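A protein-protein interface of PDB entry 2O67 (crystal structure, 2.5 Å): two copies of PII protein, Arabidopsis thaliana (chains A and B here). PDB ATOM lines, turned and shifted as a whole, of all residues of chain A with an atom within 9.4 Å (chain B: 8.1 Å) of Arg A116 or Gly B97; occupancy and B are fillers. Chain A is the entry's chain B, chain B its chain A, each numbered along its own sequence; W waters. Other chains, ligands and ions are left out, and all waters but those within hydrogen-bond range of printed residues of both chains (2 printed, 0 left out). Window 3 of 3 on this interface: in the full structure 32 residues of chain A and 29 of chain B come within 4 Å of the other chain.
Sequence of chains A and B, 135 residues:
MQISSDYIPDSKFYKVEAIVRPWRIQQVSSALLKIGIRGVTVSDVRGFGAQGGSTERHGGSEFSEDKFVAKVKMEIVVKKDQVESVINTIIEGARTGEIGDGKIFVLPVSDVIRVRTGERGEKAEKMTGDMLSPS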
ATOM      1  N   ILE A 113       4.887  16.914  -7.619  1.00  0.00           N
ATOM      2  CA  ILE A 113       4.142  16.594  -6.407  1.00  0.00           C
ATOM      3  C   ILE A 113       4.575  17.506  -5.251  1.00  0.00           C
ATOM      4  O   ILE A 113       5.769  17.661  -4.992  1.00  0.00           O
ATOM      5  CB  ILE A 113       4.330  15.094  -5.983  1.00  0.00           C
ATOM      6  CG1 ILE A 113       4.077  14.120  -7.148  1.00  0.00           C
ATOM      7  CG2 ILE A 113       3.419  14.736  -4.814  1.00  0.00           C
ATOM      8  CD1 ILE A 113       5.298  13.806  -8.019  1.00  0.00           C
ATOM      9  N   ARG A 114       3.609  18.110  -4.563  1.00  0.00           N
ATOM     10  CA  ARG A 114       3.883  18.832  -3.318  1.00  0.00           C
ATOM     11  C   ARG A 114       3.951  17.839  -2.153  1.00  0.00           C
ATOM     12  O   ARG A 114       2.990  17.124  -1.899  1.00  0.00           O
ATOM     13  CB  ARG A 114       2.819  19.907  -3.053  1.00  0.00           C
ATOM     14  CG  ARG A 114       3.166  20.821  -1.870  1.00  0.00           C
ATOM     15  CD  ARG A 114       2.057  21.812  -1.508  1.00  0.00           C
ATOM     16  NE  ARG A 114       1.544  22.550  -2.665  1.00  0.00           N
ATOM     17  CZ  ARG A 114       2.218  23.488  -3.326  1.00  0.00           C
ATOM     18  NH1 ARG A 114       3.456  23.812  -2.964  1.00  0.00           N
ATOM     19  NH2 ARG A 114       1.656  24.095  -4.360  1.00  0.00           N
ATOM     20  N   VAL A 115       5.088  17.798  -1.456  1.00  0.00           N
ATOM     21  CA  VAL A 115       5.325  16.811  -0.390  1.00  0.00           C
ATOM     22  C   VAL A 115       4.302  16.927   0.741  1.00  0.00           C
ATOM     23  O   VAL A 115       3.727  15.923   1.172  1.00  0.00           O
ATOM     24  CB  VAL A 115       6.770  16.907   0.190  1.00  0.00           C
ATOM     25  CG1 VAL A 115       6.910  16.089   1.464  1.00  0.00           C
ATOM     26  CG2 VAL A 115       7.798  16.448  -0.833  1.00  0.00           C
ATOM     27  N   ARG A 116       4.080  18.160   1.197  1.00  0.00           N
ATOM     28  CA  ARG A 116       3.227  18.459   2.352  1.00  0.00           C
ATOM     29  C   ARG A 116       1.773  18.004   2.174  1.00  0.00           C
ATOM     30  O   ARG A 116       1.167  17.470   3.108  1.00  0.00           O
ATOM     31  CB  ARG A 116       3.285  19.960   2.654  1.00  0.00           C
ATOM     32  CG  ARG A 116       2.417  20.429   3.809  1.00  0.00           C
ATOM     33  CD  ARG A 116       2.659  21.902   4.142  1.00  0.00           C
ATOM     34  NE  ARG A 116       2.346  22.815   3.042  1.00  0.00           N
ATOM     35  CZ  ARG A 116       1.118  23.199   2.708  1.00  0.00           C
ATOM     36  NH1 ARG A 116       0.063  22.740   3.376  1.00  0.00           N
ATOM     37  NH2 ARG A 116       0.943  24.040   1.697  1.00  0.00           N
ATOM     38  N   THR A 117       1.230  18.204   0.975  1.00  0.00           N
ATOM     39  CA  THR A 117      -0.188  17.968   0.718  1.00  0.00           C
ATOM     40  C   THR A 117      -0.476  16.736  -0.153  1.00  0.00           C
ATOM     41  O   THR A 117      -1.570  16.184  -0.097  1.00  0.00           O
ATOM     42  CB  THR A 117      -0.836  19.195   0.063  1.00  0.00           C
ATOM     43  OG1 THR A 117      -0.239  19.413  -1.218  1.00  0.00           O
ATOM     44  CG2 THR A 117      -0.641  20.439   0.923  1.00  0.00           C
ATOM     45  N   GLY A 118       0.498  16.316  -0.958  1.00  0.00           N
ATOM     46  CA  GLY A 118       0.314  15.205  -1.894  1.00  0.00           C
ATOM     47  C   GLY A 118      -0.273  15.630  -3.230  1.00  0.00           C
ATOM     48  O   GLY A 118      -0.524  14.790  -4.099  1.00  0.00           O
ATOM     49  N   GLU A 119      -0.486  16.935  -3.390  1.00  0.00           N
ATOM     50  CA  GLU A 119      -1.045  17.519  -4.606  1.00  0.00           C
ATOM     51  C   GLU A 119      -0.125  17.295  -5.797  1.00  0.00           C
ATOM     52  O   GLU A 119       1.098  17.380  -5.668  1.00  0.00           O
ATOM     53  CB  GLU A 119      -1.264  19.023  -4.420  1.00  0.00           C
ATOM     54  CG  GLU A 119      -2.447  19.394  -3.531  1.00  0.00           C
ATOM     55  CD  GLU A 119      -2.429  20.856  -3.124  1.00  0.00           C
ATOM     56  OE1 GLU A 119      -1.452  21.285  -2.464  1.00  0.00           O
ATOM     57  OE2 GLU A 119      -3.397  21.576  -3.462  1.00  0.00           O
ATOM     58  N   LYS A 123      -1.859  22.068  -9.463  1.00  0.00           N
ATOM     59  CA  LYS A 123      -2.074  22.475  -8.069  1.00  0.00           C
ATOM     60  C   LYS A 123      -0.870  22.131  -7.181  1.00  0.00           C
ATOM     61  O   LYS A 123      -1.015  21.924  -5.976  1.00  0.00           O
ATOM     62  CB  LYS A 123      -3.367  21.854  -7.515  1.00  0.00           C
ATOM     63  CG  LYS A 123      -4.555  21.957  -8.464  1.00  0.00           C
ATOM     64  CD  LYS A 123      -5.810  22.416  -7.751  1.00  0.00           C
ATOM     65  CE  LYS A 123      -6.783  23.043  -8.741  1.00  0.00           C
ATOM     66  NZ  LYS A 123      -7.723  23.989  -8.079  1.00  0.00           N
ATOM     67  N   ALA A 124       0.315  22.092  -7.789  1.00  0.00           N
ATOM     68  CA  ALA A 124       1.542  21.665  -7.114  1.00  0.00           C
ATOM     69  C   ALA A 124       2.792  22.383  -7.630  1.00  0.00           C
ATOM     70  O   ALA A 124       3.827  22.387  -6.956  1.00  0.00           O
ATOM     71  CB  ALA A 124       1.711  20.159  -7.244  1.00  0.00           C
ATOM     72  N   LYS A 126       3.390  25.717  -8.278  1.00  0.00           N
ATOM     73  CA  LYS A 126       3.714  26.992  -7.630  1.00  0.00           C
ATOM     74  C   LYS A 126       4.443  26.749  -6.311  1.00  0.00           C
ATOM     75  O   LYS A 126       4.026  25.909  -5.508  1.00  0.00           O
ATOM     76  CB  LYS A 126       2.453  27.836  -7.379  1.00  0.00           C
ATOM     77  CG  LYS A 126       1.288  27.622  -8.354  1.00  0.00           C
ATOM     78  CD  LYS A 126       1.506  28.305  -9.704  1.00  0.00           C
ATOM     79  CE  LYS A 126       0.332  28.047 -10.649  1.00  0.00           C
ATOM     80  NZ  LYS A 126       0.540  28.667 -11.992  1.00  0.00           N
ATOM     81  N   MET A 127       5.538  27.476  -6.105  1.00  0.00           N
ATOM     82  CA  MET A 127       6.276  27.425  -4.846  1.00  0.00           C
ATOM     83  C   MET A 127       5.528  28.243  -3.799  1.00  0.00           C
ATOM     84  O   MET A 127       5.240  29.426  -4.010  1.00  0.00           O
ATOM     85  CB  MET A 127       7.707  27.938  -5.031  1.00  0.00           C
ATOM     86  CG  MET A 127       8.584  27.031  -5.892  1.00  0.00           C
ATOM     87  SD  MET A 127       9.548  25.818  -4.959  1.00  0.00           S
ATOM     88  CE  MET A 127      10.336  24.889  -6.280  1.00  0.00           C
ATOM     89  N   THR A 128       5.203  27.591  -2.684  1.00  0.00           N
ATOM     90  CA  THR A 128       4.378  28.179  -1.625  1.00  0.00           C
ATOM     91  C   THR A 128       5.138  28.285  -0.300  1.00  0.00           C
ATOM     92  O   THR A 128       4.564  28.094   0.776  1.00  0.00           O
ATOM     93  CB  THR A 128       3.068  27.373  -1.409  1.00  0.00           C
ATOM     94  OG1 THR A 128       3.382  25.999  -1.155  1.00  0.00           O
ATOM     95  CG2 THR A 128       2.158  27.465  -2.624  1.00  0.00           C
ATOM     96  N   GLY A 129       6.434  28.579  -0.387  1.00  0.00           N
ATOM     97  CA  GLY A 129       7.258  28.813   0.796  1.00  0.00           C
ATOM     98  C   GLY A 129       7.255  30.280   1.190  1.00  0.00           C
ATOM     99  O   GLY A 129       6.805  31.135   0.421  1.00  0.00           O
ATOM    100  N   ARG B  21      13.571  18.705   3.294  1.00  0.00           N
ATOM    101  CA  ARG B  21      14.301  19.232   4.455  1.00  0.00           C
ATOM    102  C   ARG B  21      15.525  18.372   4.759  1.00  0.00           C
ATOM    103  O   ARG B  21      15.421  17.145   4.774  1.00  0.00           O
ATOM    104  CB  ARG B  21      13.399  19.268   5.706  1.00  0.00           C
ATOM    105  CG  ARG B  21      12.096  20.067   5.575  1.00  0.00           C
ATOM    106  CD  ARG B  21      11.143  19.795   6.765  1.00  0.00           C
ATOM    107  NE  ARG B  21       9.809  20.359   6.539  1.00  0.00           N
ATOM    108  CZ  ARG B  21       9.461  21.616   6.822  1.00  0.00           C
ATOM    109  NH1 ARG B  21      10.341  22.452   7.350  1.00  0.00           N
ATOM    110  NH2 ARG B  21       8.233  22.050   6.567  1.00  0.00           N
ATOM    111  N   ARG B  24      15.485  15.325   7.145  1.00  0.00           N
ATOM    112  CA  ARG B  24      14.637  14.198   6.741  1.00  0.00           C
ATOM    113  C   ARG B  24      15.347  13.210   5.806  1.00  0.00           C
ATOM    114  O   ARG B  24      14.693  12.337   5.224  1.00  0.00           O
ATOM    115  CB  ARG B  24      13.346  14.690   6.065  1.00  0.00           C
ATOM    116  CG  ARG B  24      12.505  15.664   6.877  1.00  0.00           C
ATOM    117  CD  ARG B  24      12.030  15.082   8.200  1.00  0.00           C
ATOM    118  NE  ARG B  24      11.212  13.884   8.031  1.00  0.00           N
ATOM    119  CZ  ARG B  24      10.442  13.356   8.978  1.00  0.00           C
ATOM    120  NH1 ARG B  24      10.367  13.921  10.176  1.00  0.00           N
ATOM    121  NH2 ARG B  24       9.739  12.261   8.722  1.00  0.00           N
ATOM    122  N   ILE B  91       7.211  10.948   0.293  1.00  0.00           N
ATOM    123  CA  ILE B  91       6.234  11.739   1.056  1.00  0.00           C
ATOM    124  C   ILE B  91       6.213  11.289   2.524  1.00  0.00           C
ATOM    125  O   ILE B  91       6.337  12.109   3.427  1.00  0.00           O
ATOM    126  CB  ILE B  91       4.807  11.674   0.449  1.00  0.00           C
ATOM    127  CG1 ILE B  91       4.778  12.340  -0.932  1.00  0.00           C
ATOM    128  CG2 ILE B  91       3.806  12.354   1.373  1.00  0.00           C
ATOM    129  CD1 ILE B  91       3.466  12.177  -1.689  1.00  0.00           C
ATOM    130  N   ALA B  94       9.389  12.270   4.267  1.00  0.00           N
ATOM    131  CA  ALA B  94       9.714  13.702   4.215  1.00  0.00           C
ATOM    132  C   ALA B  94       8.647  14.658   4.775  1.00  0.00           C
ATOM    133  O   ALA B  94       8.967  15.795   5.139  1.00  0.00           O
ATOM    134  CB  ALA B  94      10.076  14.105   2.792  1.00  0.00           C
ATOM    135  N   ARG B  95       7.392  14.210   4.820  1.00  0.00           N
ATOM    136  CA  ARG B  95       6.285  15.054   5.278  1.00  0.00           C
ATOM    137  C   ARG B  95       6.359  15.344   6.781  1.00  0.00           C
ATOM    138  O   ARG B  95       6.535  14.429   7.593  1.00  0.00           O
ATOM    139  CB  ARG B  95       4.938  14.427   4.917  1.00  0.00           C
ATOM    140  CG  ARG B  95       3.736  15.144   5.510  1.00  0.00           C
ATOM    141  CD  ARG B  95       2.677  15.385   4.464  1.00  0.00           C
ATOM    142  NE  ARG B  95       1.896  14.191   4.185  1.00  0.00           N
ATOM    143  CZ  ARG B  95       1.264  13.942   3.039  1.00  0.00           C
ATOM    144  NH1 ARG B  95       1.333  14.789   2.016  1.00  0.00           N
ATOM    145  NH2 ARG B  95       0.574  12.818   2.908  1.00  0.00           N
ATOM    146  N   THR B  96       6.259  16.628   7.126  1.00  0.00           N
ATOM    147  CA  THR B  96       6.082  17.065   8.513  1.00  0.00           C
ATOM    148  C   THR B  96       4.708  17.716   8.646  1.00  0.00           C
ATOM    149  O   THR B  96       4.146  17.776   9.736  1.00  0.00           O
ATOM    150  CB  THR B  96       7.174  18.064   8.979  1.00  0.00           C
ATOM    151  OG1 THR B  96       6.996  19.322   8.314  1.00  0.00           O
ATOM    152  CG2 THR B  96       8.578  17.527   8.708  1.00  0.00           C
ATOM    153  N   GLY B  97       4.175  18.188   7.521  1.00  0.00           N
ATOM    154  CA  GLY B  97       2.878  18.852   7.478  1.00  0.00           C
ATOM    155  C   GLY B  97       2.968  20.371   7.434  1.00  0.00           C
ATOM    156  O   GLY B  97       1.961  21.053   7.230  1.00  0.00           O
ATOM    157  N   GLU B  98       4.172  20.899   7.630  1.00  0.00           N
ATOM    158  CA  GLU B  98       4.402  22.343   7.627  1.00  0.00           C
ATOM    159  C   GLU B  98       4.978  22.842   6.297  1.00  0.00           C
ATOM    160  O   GLU B  98       5.670  22.099   5.588  1.00  0.00           O
ATOM    161  CB  GLU B  98       5.336  22.737   8.777  1.00  0.00           C
ATOM    162  CG  GLU B  98       4.740  22.533  10.169  1.00  0.00           C
ATOM    163  CD  GLU B  98       5.718  22.845  11.290  1.00  0.00           C
ATOM    164  OE1 GLU B  98       6.914  23.068  11.005  1.00  0.00           O
ATOM    165  OE2 GLU B  98       5.292  22.866  12.467  1.00  0.00           O
ATOM    166  N   ILE B  99       4.668  24.097   5.970  1.00  0.00           N
ATOM    167  CA  ILE B  99       5.248  24.797   4.826  1.00  0.00           C
ATOM    168  C   ILE B  99       6.769  24.606   4.817  1.00  0.00           C
ATOM    169  O   ILE B  99       7.434  24.822   5.834  1.00  0.00           O
ATOM    170  CB  ILE B  99       4.901  26.315   4.845  1.00  0.00           C
ATOM    171  CG1 ILE B  99       3.393  26.544   4.684  1.00  0.00           C
ATOM    172  CG2 ILE B  99       5.682  27.072   3.769  1.00  0.00           C
ATOM    173  CD1 ILE B  99       2.864  26.404   3.263  1.00  0.00           C
ATOM    174  N   GLY B 100       7.299  24.173   3.673  1.00  0.00           N
ATOM    175  CA  GLY B 100       8.734  23.952   3.509  1.00  0.00           C
ATOM    176  C   GLY B 100       9.136  22.491   3.448  1.00  0.00           C
ATOM    177  O   GLY B 100      10.321  22.167   3.573  1.00  0.00           O
ATOM    178  N   ASP B 101       8.149  21.616   3.261  1.00  0.00           N
ATOM    179  CA  ASP B 101       8.369  20.175   3.139  1.00  0.00           C
ATOM    180  C   ASP B 101       9.076  19.804   1.834  1.00  0.00           C
ATOM    181  O   ASP B 101       9.831  18.834   1.792  1.00  0.00           O
ATOM    182  CB  ASP B 101       7.040  19.415   3.241  1.00  0.00           C
ATOM    183  CG  ASP B 101       6.611  19.148   4.685  1.00  0.00           C
ATOM    184  OD1 ASP B 101       7.392  19.419   5.630  1.00  0.00           O
ATOM    185  OD2 ASP B 101       5.480  18.660   4.869  1.00  0.00           O
ATOM    186  N   GLY B 102       8.804  20.566   0.774  1.00  0.00           N
ATOM    187  CA  GLY B 102       9.484  20.407  -0.502  1.00  0.00           C
ATOM    188  C   GLY B 102       8.608  19.943  -1.651  1.00  0.00           C
ATOM    189  O   GLY B 102       7.372  19.970  -1.568  1.00  0.00           O
ATOM    190  N   LYS B 103       9.263  19.523  -2.732  1.00  0.00           N
ATOM    191  CA  LYS B 103       8.581  19.033  -3.927  1.00  0.00           C
ATOM    192  C   LYS B 103       9.242  17.773  -4.455  1.00  0.00           C
ATOM    193  O   LYS B 103      10.405  17.495  -4.154  1.00  0.00           O
ATOM    194  CB  LYS B 103       8.570  20.092  -5.032  1.00  0.00           C
ATOM    195  CG  LYS B 103       7.651  21.278  -4.766  1.00  0.00           C
ATOM    196  CD  LYS B 103       7.114  21.858  -6.068  1.00  0.00           C
ATOM    197  CE  LYS B 103       6.799  23.335  -5.939  1.00  0.00           C
ATOM    198  NZ  LYS B 103       5.598  23.589  -5.116  1.00  0.00           N
ATOM    199  N   ILE B 104       8.488  17.017  -5.246  1.00  0.00           N
ATOM    200  CA  ILE B 104       9.014  15.848  -5.945  1.00  0.00           C
ATOM    201  C   ILE B 104       8.806  16.071  -7.431  1.00  0.00           C
ATOM    202  O   ILE B 104       7.712  16.442  -7.859  1.00  0.00           O
ATOM    203  CB  ILE B 104       8.317  14.526  -5.510  1.00  0.00           C
ATOM    204  CG1 ILE B 104       8.594  14.227  -4.034  1.00  0.00           C
ATOM    205  CG2 ILE B 104       8.781  13.362  -6.384  1.00  0.00           C
ATOM    206  CD1 ILE B 104       7.592  13.296  -3.400  1.00  0.00           C
HETATM  207  O   HOH W   1       5.418  20.432   0.275  1.00  0.00           O
HETATM  208  O   HOH W   2      -0.346  21.147   5.585  1.00  0.00           O
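Of the printed residues of chain B, Ile A113 touches Lys B103 and Ile B104. Of the printed residues of chain B, Arg A114 touches Lys B103. Arg A116 touches just these residues of chain B: Arg B95, Gly B97, Glu B98, Ile B99 and Asp B101. Glu A119 touches none of the printed residues of chain B. Of the printed residues of chain B, Ala A124 touches Lys B103. Printed residues of chain B within 4 Å of Thr A128: Ile B99 (3.4 Å). Arg B21 touches none of the printed residues of chain A. No residue of chain A comes within 4 Å of Thr B96. Gly B97 touches just one residue of chain A: Arg A116. Of the printed residues of chain A, Ile B104 touches Ile A113 (2.8 Å) and Val A115 (3.98 Å). The nearest residue of chain B that does not touch Arg A116 is Gly B102 (4.7 Å). The nearest printed residue of chain A that does not touch Gly B97 is Thr A117 (6.7 Å).
Water W1 lies within hydrogen-bond range of O of Gly B102, N of Arg A116 and N of Val A115. Water W2 lies within hydrogen-bond range of the guanidinium group (NH1) of Arg A116 (2.8 Å) and the backbone carbonyl oxygen (O) of Gly B97 (2.8 Å).
Of the 14 printed residues of chain B, 10 touch a printed residue of chain A. Hydrophobic or aromatic side chains of chain B that line the printed part of chain A: Ile B91, Ala B94, Ile B99 and Ile B104. Hydrophobic or aromatic side chains of chain A within 4 Å of the printed part of chain B: Ile A113, Val A115 and Met A127. Along chain A the printed residues that touch a printed residue of chain B span positions 113 to 129. Among the printed residues, 22 pairs touch across the chains.
No position is printed for both chains.
The side-chain hydroxyl of Thr A117 is in hydrogen-bond range of the side-chain carboxylate of Glu A119, at 2.6 Å. The guanidinium group (NH2) of Arg B21 sits at hydrogen-bond distance from the backbone carbonyl oxygen (O) of Glu B98 (2.7 Å). NE of Arg B21 lies within salt-bridge range of OD1 of Asp B101 (2.7 Å). O of Ile B99 is in hydrogen-bond range of NH2 of Arg B21, at 3.0 Å. The side-chain carboxylate (OD2) of Asp B101 lies within hydrogen-bond range of the backbone NH (N) of Gly B97. The side-chain hydroxyl of Thr A128 sits at hydrogen-bond distance from the guanidinium group of Arg A114.
CA of Lys B103 touches O of Ile A113, at 3.3 Å. Val A115 touches Ala B94 (CG1 to CB, 3.97 Å). Ile B104 touches Val A115 (CG1 to CG2, 3.98 Å). O of Gly B97 touches CD of Arg A116, at 3.3 Å. Arg A116 touches Glu B98 (CD to C, 3.3 Å). Arg A116 touches Ile B99. Arg B95 touches Thr A117 (NH1 to C, 3.4 Å). Lys B103 touches Met A127. Ile B99 touches Thr A128 (CG2 to O, 3.4 Å). CG2 of Ile B99 touches CA of Gly A129, at 3.8 Å.
O of Ala A124 is in hydrogen-bond range of NZ of Lys B103, 2.8 Å away. N of Ile B104 sits at hydrogen-bond distance from O of Ile A113, 2.8 Å away. The backbone NH (N) of Gly A118 sits close to the guanidinium group (NH1) of Arg B95, 3.4 Å away. The backbone carbonyl oxygen of Gly B102 sits at hydrogen-bond distance from the backbone NH of Val A115. The side-chain amino group of Lys B103 sits at hydrogen-bond distance from the backbone carbonyl oxygen of Lys A126, at 2.8 Å. The guanidinium group of Arg A114 sits close to the side-chain amino group of Lys B103, 3.0 Å away. NH1 of Arg B95 lies within hydrogen-bond range of O of Arg A116. The guanidinium group (NH1) of Arg B95 is in hydrogen-bond range of the backbone carbonyl oxygen (O) of Val A115, at 2.8 Å.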
